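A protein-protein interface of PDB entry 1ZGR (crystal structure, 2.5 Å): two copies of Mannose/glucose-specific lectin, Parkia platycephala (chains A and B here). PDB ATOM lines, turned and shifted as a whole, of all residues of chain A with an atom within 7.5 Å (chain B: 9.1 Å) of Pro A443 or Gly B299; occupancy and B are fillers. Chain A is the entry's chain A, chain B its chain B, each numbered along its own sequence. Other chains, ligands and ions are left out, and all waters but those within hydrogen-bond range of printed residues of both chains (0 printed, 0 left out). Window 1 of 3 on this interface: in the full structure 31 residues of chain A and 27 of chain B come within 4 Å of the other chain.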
ATOM      1  N   GLY A 299      21.423   3.393   1.087  1.00  0.00           N
ATOM      2  CA  GLY A 299      20.599   2.290   0.403  1.00  0.00           C
ATOM      3  C   GLY A 299      20.303   2.576  -1.094  1.00  0.00           C
ATOM      4  O   GLY A 299      20.862   1.919  -1.974  1.00  0.00           O
ATOM      5  N   SER A 300      19.450   3.550  -1.420  1.00  0.00           N
ATOM      6  CA  SER A 300      18.827   3.472  -2.756  1.00  0.00           C
ATOM      7  C   SER A 300      19.380   4.376  -3.910  1.00  0.00           C
ATOM      8  O   SER A 300      19.720   5.537  -3.696  1.00  0.00           O
ATOM      9  CB  SER A 300      17.312   3.553  -2.583  1.00  0.00           C
ATOM     10  OG  SER A 300      16.767   4.415  -3.548  1.00  0.00           O
ATOM     11  N   ILE A 301      19.473   3.829  -5.127  1.00  0.00           N
ATOM     12  CA  ILE A 301      19.854   4.610  -6.319  1.00  0.00           C
ATOM     13  C   ILE A 301      18.705   5.464  -6.860  1.00  0.00           C
ATOM     14  O   ILE A 301      17.574   5.015  -6.933  1.00  0.00           O
ATOM     15  CB  ILE A 301      20.378   3.697  -7.442  1.00  0.00           C
ATOM     16  CG1 ILE A 301      21.670   3.003  -7.001  1.00  0.00           C
ATOM     17  CG2 ILE A 301      20.575   4.490  -8.735  1.00  0.00           C
ATOM     18  CD1 ILE A 301      22.066   1.837  -7.872  1.00  0.00           C
ATOM     19  N   HIS A 419      18.040  -3.052 -16.070  1.00  0.00           N
ATOM     20  CA  HIS A 419      17.757  -4.460 -15.824  1.00  0.00           C
ATOM     21  C   HIS A 419      18.229  -4.821 -14.450  1.00  0.00           C
ATOM     22  O   HIS A 419      19.103  -4.145 -13.884  1.00  0.00           O
ATOM     23  CB  HIS A 419      18.485  -5.352 -16.843  1.00  0.00           C
ATOM     24  CG  HIS A 419      18.219  -4.972 -18.259  1.00  0.00           C
ATOM     25  ND1 HIS A 419      17.242  -5.572 -19.011  1.00  0.00           N
ATOM     26  CD2 HIS A 419      18.772  -4.014 -19.048  1.00  0.00           C
ATOM     27  CE1 HIS A 419      17.216  -5.017 -20.215  1.00  0.00           C
ATOM     28  NE2 HIS A 419      18.130  -4.063 -20.258  1.00  0.00           N
ATOM     29  N   ASN A 420      17.654  -5.903 -13.943  1.00  0.00           N
ATOM     30  CA  ASN A 420      18.025  -6.532 -12.679  1.00  0.00           C
ATOM     31  C   ASN A 420      17.734  -5.623 -11.485  1.00  0.00           C
ATOM     32  O   ASN A 420      18.441  -5.644 -10.471  1.00  0.00           O
ATOM     33  CB  ASN A 420      19.475  -7.107 -12.690  1.00  0.00           C
ATOM     34  CG  ASN A 420      19.751  -8.045 -11.474  1.00  0.00           C
ATOM     35  OD1 ASN A 420      18.903  -8.879 -11.094  1.00  0.00           O
ATOM     36  ND2 ASN A 420      20.939  -7.881 -10.839  1.00  0.00           N
ATOM     37  N   ASN A 421      16.639  -4.868 -11.604  1.00  0.00           N
ATOM     38  CA  ASN A 421      16.280  -3.834 -10.626  1.00  0.00           C
ATOM     39  C   ASN A 421      14.812  -3.873 -10.261  1.00  0.00           C
ATOM     40  O   ASN A 421      14.001  -4.437 -10.983  1.00  0.00           O
ATOM     41  CB  ASN A 421      16.581  -2.439 -11.197  1.00  0.00           C
ATOM     42  CG  ASN A 421      15.566  -2.024 -12.244  1.00  0.00           C
ATOM     43  OD1 ASN A 421      15.433  -2.673 -13.260  1.00  0.00           O
ATOM     44  ND2 ASN A 421      14.809  -0.962 -11.971  1.00  0.00           N
ATOM     45  N   MET A 422      14.462  -3.254  -9.140  1.00  0.00           N
ATOM     46  CA  MET A 422      13.054  -2.993  -8.855  1.00  0.00           C
ATOM     47  C   MET A 422      12.930  -1.532  -8.465  1.00  0.00           C
ATOM     48  O   MET A 422      13.907  -0.952  -8.037  1.00  0.00           O
ATOM     49  CB  MET A 422      12.552  -3.933  -7.759  1.00  0.00           C
ATOM     50  CG  MET A 422      13.477  -4.065  -6.572  1.00  0.00           C
ATOM     51  SD  MET A 422      12.995  -5.409  -5.437  1.00  0.00           S
ATOM     52  CE  MET A 422      13.763  -4.756  -3.928  1.00  0.00           C
ATOM     53  N   VAL A 424      11.537   1.290  -5.993  1.00  0.00           N
ATOM     54  CA  VAL A 424      11.030   1.315  -4.596  1.00  0.00           C
ATOM     55  C   VAL A 424      10.372   2.628  -4.228  1.00  0.00           C
ATOM     56  O   VAL A 424       9.738   2.735  -3.175  1.00  0.00           O
ATOM     57  CB  VAL A 424      12.096   0.921  -3.506  1.00  0.00           C
ATOM     58  CG1 VAL A 424      12.536  -0.546  -3.698  1.00  0.00           C
ATOM     59  CG2 VAL A 424      13.331   1.875  -3.518  1.00  0.00           C
ATOM     60  N   VAL A 441      15.554   3.073  -7.250  1.00  0.00           N
ATOM     61  CA  VAL A 441      15.701   1.650  -7.574  1.00  0.00           C
ATOM     62  C   VAL A 441      16.688   0.946  -6.651  1.00  0.00           C
ATOM     63  O   VAL A 441      17.596   1.565  -6.087  1.00  0.00           O
ATOM     64  CB  VAL A 441      16.166   1.408  -9.008  1.00  0.00           C
ATOM     65  CG1 VAL A 441      15.234   2.048 -10.001  1.00  0.00           C
ATOM     66  CG2 VAL A 441      17.540   1.967  -9.199  1.00  0.00           C
ATOM     67  N   LYS A 442      16.461  -0.352  -6.501  1.00  0.00           N
ATOM     68  CA  LYS A 442      17.346  -1.287  -5.828  1.00  0.00           C
ATOM     69  C   LYS A 442      17.576  -2.458  -6.773  1.00  0.00           C
ATOM     70  O   LYS A 442      16.800  -2.673  -7.681  1.00  0.00           O
ATOM     71  CB  LYS A 442      16.742  -1.753  -4.491  1.00  0.00           C
ATOM     72  CG  LYS A 442      16.849  -0.625  -3.411  1.00  0.00           C
ATOM     73  CD  LYS A 442      16.630  -1.137  -1.953  1.00  0.00           C
ATOM     74  CE  LYS A 442      17.060  -0.036  -0.975  1.00  0.00           C
ATOM     75  NZ  LYS A 442      17.796  -0.579   0.229  1.00  0.00           N
ATOM     76  N   PRO A 443      18.669  -3.186  -6.614  1.00  0.00           N
ATOM     77  CA  PRO A 443      18.844  -4.422  -7.364  1.00  0.00           C
ATOM     78  C   PRO A 443      17.718  -5.442  -7.091  1.00  0.00           C
ATOM     79  O   PRO A 443      17.214  -5.506  -5.966  1.00  0.00           O
ATOM     80  CB  PRO A 443      20.193  -4.952  -6.866  1.00  0.00           C
ATOM     81  CG  PRO A 443      20.478  -4.188  -5.580  1.00  0.00           C
ATOM     82  CD  PRO A 443      19.837  -2.869  -5.763  1.00  0.00           C
ATOM     83  N   ASP A 444      17.291  -6.152  -8.149  1.00  0.00           N
ATOM     84  CA  ASP A 444      16.488  -7.407  -8.094  1.00  0.00           C
ATOM     85  C   ASP A 444      15.476  -7.749  -9.214  1.00  0.00           C
ATOM     86  O   ASP A 444      14.282  -7.989  -8.980  1.00  0.00           O
ATOM     87  CB  ASP A 444      15.857  -7.662  -6.736  1.00  0.00           C
ATOM     88  CG  ASP A 444      16.338  -8.929  -6.143  1.00  0.00           C
ATOM     89  OD1 ASP A 444      17.460  -9.332  -6.539  1.00  0.00           O
ATOM     90  OD2 ASP A 444      15.678  -9.600  -5.306  1.00  0.00           O
ATOM     91  N   ARG B 295      30.367 -14.991  -4.936  1.00  0.00           N
ATOM     92  CA  ARG B 295      29.123 -14.621  -5.648  1.00  0.00           C
ATOM     93  C   ARG B 295      28.310 -13.630  -4.783  1.00  0.00           C
ATOM     94  O   ARG B 295      27.885 -13.990  -3.679  1.00  0.00           O
ATOM     95  CB  ARG B 295      28.262 -15.872  -5.850  1.00  0.00           C
ATOM     96  CG  ARG B 295      28.496 -16.655  -7.099  1.00  0.00           C
ATOM     97  CD  ARG B 295      27.722 -16.144  -8.293  1.00  0.00           C
ATOM     98  NE  ARG B 295      26.327 -16.558  -8.252  1.00  0.00           N
ATOM     99  CZ  ARG B 295      25.439 -16.296  -9.212  1.00  0.00           C
ATOM    100  NH1 ARG B 295      25.786 -15.617 -10.308  1.00  0.00           N
ATOM    101  NH2 ARG B 295      24.197 -16.721  -9.076  1.00  0.00           N
ATOM    102  N   ASP B 296      28.078 -12.406  -5.262  1.00  0.00           N
ATOM    103  CA  ASP B 296      27.544 -11.323  -4.379  1.00  0.00           C
ATOM    104  C   ASP B 296      26.083 -11.481  -3.844  1.00  0.00           C
ATOM    105  O   ASP B 296      25.296 -12.338  -4.299  1.00  0.00           O
ATOM    106  CB  ASP B 296      27.752  -9.923  -5.009  1.00  0.00           C
ATOM    107  CG  ASP B 296      26.880  -9.700  -6.262  1.00  0.00           C
ATOM    108  OD1 ASP B 296      26.431 -10.706  -6.885  1.00  0.00           O
ATOM    109  OD2 ASP B 296      26.589  -8.546  -6.690  1.00  0.00           O
ATOM    110  N   GLY B 299      23.073  -7.666  -5.143  1.00  0.00           N
ATOM    111  CA  GLY B 299      22.982  -7.849  -6.616  1.00  0.00           C
ATOM    112  C   GLY B 299      23.531  -6.644  -7.388  1.00  0.00           C
ATOM    113  O   GLY B 299      23.972  -5.664  -6.760  1.00  0.00           O
ATOM    114  N   SER B 300      23.536  -6.692  -8.721  1.00  0.00           N
ATOM    115  CA  SER B 300      24.046  -5.539  -9.482  1.00  0.00           C
ATOM    116  C   SER B 300      23.197  -5.052 -10.675  1.00  0.00           C
ATOM    117  O   SER B 300      22.857  -5.798 -11.591  1.00  0.00           O
ATOM    118  CB  SER B 300      25.542  -5.715  -9.833  1.00  0.00           C
ATOM    119  OG  SER B 300      25.833  -5.211 -11.122  1.00  0.00           O
ATOM    120  N   ILE B 301      22.862  -3.775 -10.651  1.00  0.00           N
ATOM    121  CA  ILE B 301      21.992  -3.229 -11.666  1.00  0.00           C
ATOM    122  C   ILE B 301      22.730  -2.921 -12.946  1.00  0.00           C
ATOM    123  O   ILE B 301      23.824  -2.348 -12.941  1.00  0.00           O
ATOM    124  CB  ILE B 301      21.292  -1.985 -11.150  1.00  0.00           C
ATOM    125  CG1 ILE B 301      20.256  -2.383 -10.122  1.00  0.00           C
ATOM    126  CG2 ILE B 301      20.650  -1.215 -12.291  1.00  0.00           C
ATOM    127  CD1 ILE B 301      19.935  -1.211  -9.178  1.00  0.00           C
ATOM    128  N   SER B 302      22.093  -3.258 -14.053  1.00  0.00           N
ATOM    129  CA  SER B 302      22.655  -3.008 -15.360  1.00  0.00           C
ATOM    130  C   SER B 302      21.949  -1.821 -16.020  1.00  0.00           C
ATOM    131  O   SER B 302      20.724  -1.739 -15.994  1.00  0.00           O
ATOM    132  CB  SER B 302      22.466  -4.268 -16.198  1.00  0.00           C
ATOM    133  OG  SER B 302      23.135  -4.131 -17.421  1.00  0.00           O
ATOM    134  N   MET B 422      27.591   3.744  -7.402  1.00  0.00           N
ATOM    135  CA  MET B 422      28.934   3.610  -7.943  1.00  0.00           C
ATOM    136  C   MET B 422      28.934   2.597  -9.097  1.00  0.00           C
ATOM    137  O   MET B 422      28.203   1.591  -9.063  1.00  0.00           O
ATOM    138  CB  MET B 422      29.949   3.262  -6.837  1.00  0.00           C
ATOM    139  CG  MET B 422      29.785   1.881  -6.214  1.00  0.00           C
ATOM    140  SD  MET B 422      30.324   1.818  -4.484  1.00  0.00           S
ATOM    141  CE  MET B 422      32.100   2.110  -4.677  1.00  0.00           C
ATOM    142  N   VAL B 424      30.492  -0.387 -11.018  1.00  0.00           N
ATOM    143  CA  VAL B 424      31.328  -1.502 -10.656  1.00  0.00           C
ATOM    144  C   VAL B 424      31.797  -2.271 -11.889  1.00  0.00           C
ATOM    145  O   VAL B 424      32.418  -3.324 -11.776  1.00  0.00           O
ATOM    146  CB  VAL B 424      30.600  -2.441  -9.650  1.00  0.00           C
ATOM    147  CG1 VAL B 424      30.388  -1.734  -8.302  1.00  0.00           C
ATOM    148  CG2 VAL B 424      29.279  -2.955 -10.213  1.00  0.00           C
ATOM    149  N   PHE B 440      27.469  -1.214 -15.107  1.00  0.00           N
ATOM    150  CA  PHE B 440      26.955  -2.006 -14.002  1.00  0.00           C
ATOM    151  C   PHE B 440      27.106  -1.110 -12.785  1.00  0.00           C
ATOM    152  O   PHE B 440      28.200  -0.605 -12.521  1.00  0.00           O
ATOM    153  CB  PHE B 440      27.798  -3.262 -13.761  1.00  0.00           C
ATOM    154  CG  PHE B 440      27.637  -4.350 -14.808  1.00  0.00           C
ATOM    155  CD1 PHE B 440      28.760  -4.879 -15.451  1.00  0.00           C
ATOM    156  CD2 PHE B 440      26.374  -4.883 -15.105  1.00  0.00           C
ATOM    157  CE1 PHE B 440      28.624  -5.920 -16.384  1.00  0.00           C
ATOM    158  CE2 PHE B 440      26.221  -5.901 -16.035  1.00  0.00           C
ATOM    159  CZ  PHE B 440      27.342  -6.426 -16.689  1.00  0.00           C
ATOM    160  N   VAL B 441      26.025  -0.904 -12.037  1.00  0.00           N
ATOM    161  CA  VAL B 441      26.068  -0.001 -10.889  1.00  0.00           C
ATOM    162  C   VAL B 441      25.528  -0.694  -9.668  1.00  0.00           C
ATOM    163  O   VAL B 441      24.874  -1.733  -9.778  1.00  0.00           O
ATOM    164  CB  VAL B 441      25.281   1.322 -11.115  1.00  0.00           C
ATOM    165  CG1 VAL B 441      25.809   2.060 -12.301  1.00  0.00           C
ATOM    166  CG2 VAL B 441      23.775   1.061 -11.285  1.00  0.00           C
ATOM    167  N   LYS B 442      25.826  -0.086  -8.518  1.00  0.00           N
ATOM    168  CA  LYS B 442      25.418  -0.508  -7.175  1.00  0.00           C
ATOM    169  C   LYS B 442      25.238   0.800  -6.429  1.00  0.00           C
ATOM    170  O   LYS B 442      25.704   1.831  -6.897  1.00  0.00           O
ATOM    171  CB  LYS B 442      26.534  -1.310  -6.472  1.00  0.00           C
ATOM    172  CG  LYS B 442      26.857  -2.651  -7.104  1.00  0.00           C
ATOM    173  CD  LYS B 442      27.547  -3.559  -6.112  1.00  0.00           C
ATOM    174  CE  LYS B 442      27.308  -5.025  -6.456  1.00  0.00           C
ATOM    175  NZ  LYS B 442      28.013  -5.936  -5.495  1.00  0.00           N
ATOM    176  N   PRO B 443      24.593   0.777  -5.270  1.00  0.00           N
ATOM    177  CA  PRO B 443      24.436   2.004  -4.473  1.00  0.00           C
ATOM    178  C   PRO B 443      25.752   2.538  -3.881  1.00  0.00           C
ATOM    179  O   PRO B 443      26.680   1.753  -3.635  1.00  0.00           O
ATOM    180  CB  PRO B 443      23.493   1.579  -3.343  1.00  0.00           C
ATOM    181  CG  PRO B 443      22.896   0.262  -3.770  1.00  0.00           C
ATOM    182  CD  PRO B 443      23.936  -0.395  -4.650  1.00  0.00           C
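N of His A419 is in hydrogen-bond range of O of Ser B302, at 3.0 Å. O of Ser B300 lies within hydrogen-bond range of ND2 of Asn A420, at 2.9 Å.
The backbone NH (N) of Met A422 sits at hydrogen-bond distance from the backbone carbonyl oxygen (O) of Lys A442 (2.8 Å). The backbone NH of Met B422 is in hydrogen-bond range of the backbone carbonyl oxygen of Lys B442, 2.7 Å away. The backbone NH (N) of Val A441 lies within hydrogen-bond range of the backbone carbonyl oxygen (O) of Ile A301. NZ of Lys B442 is in salt-bridge range of OD2 of Asp B296 (3.2 Å). The backbone carbonyl oxygen of Asn A420 is in hydrogen-bond range of the backbone NH of Asp A444. O of Ile B301 lies within hydrogen-bond range of N of Val B441, at 2.8 Å.
Among the printed residues, merely in contact across the chains: Gly A299 with Pro B443, Pro A443 with Ile B301, Lys A442 with Ile B301, Ile A301 with Lys B442, His A419 with Ile B301, Asn A420 with Ile B301, Pro A443 with Gly B299, Ile A301 with Pro B443, Asn A421 with Ile B301, Ile A301 with Val B441, Ile A301 with Ile B301 and Val A441 with Ile B301.
Printed residues of chain B within 4 Å of Gly A299: Pro B443 (3.0 Å). Pro A443 touches just these residues of chain B: Gly B299 (3.8 Å) and Ile B301 (3.5 Å). No residue of chain B comes within 4 Å of Asp A444. Gly B299 touches one residue of chain A. Val B424 touches none of the printed residues of chain A. Printed residues of chain A within 4 Å of Lys B442: Ile A301 (3.6 Å). The nearest residue of chain A that does not touch Gly B299 is Asn A420 (4.5 Å). The nearest printed residue of chain B that does not touch Gly A299 is Lys B442 (6.3 Å).
Of the 12 printed residues of chain B, 7 touch a printed residue of chain A. Printed residues of chain B that touch a printed residue of chain A: Gly B299, Ser B300, Ile B301, Ser B302, Val B441, Lys B442 and Pro B443. Of the 12 printed residues of chain A, 8 touch a printed residue of chain B. Printed residues of chain A that touch a printed residue of chain B: Gly A299, Ile A301, His A419, Asn A420, Asn A421, Val A441, Lys A442 and Pro A443.
Gly A299 touches Pro B443, and with the chains exchanged Pro A443 touches Gly B299. Ile A301 touches Val B441, and with the chains exchanged Val A441 touches Ile B301. Ile A301 touches Lys B442, and with the chains exchanged Lys A442 touches Ile B301. Ile A301 touches Pro B443, and with the chains exchanged Pro A443 touches Ile B301. Of the 14 pairs that touch across the chains among the printed residues, 9 have their exchanged pair printed and touching as well.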
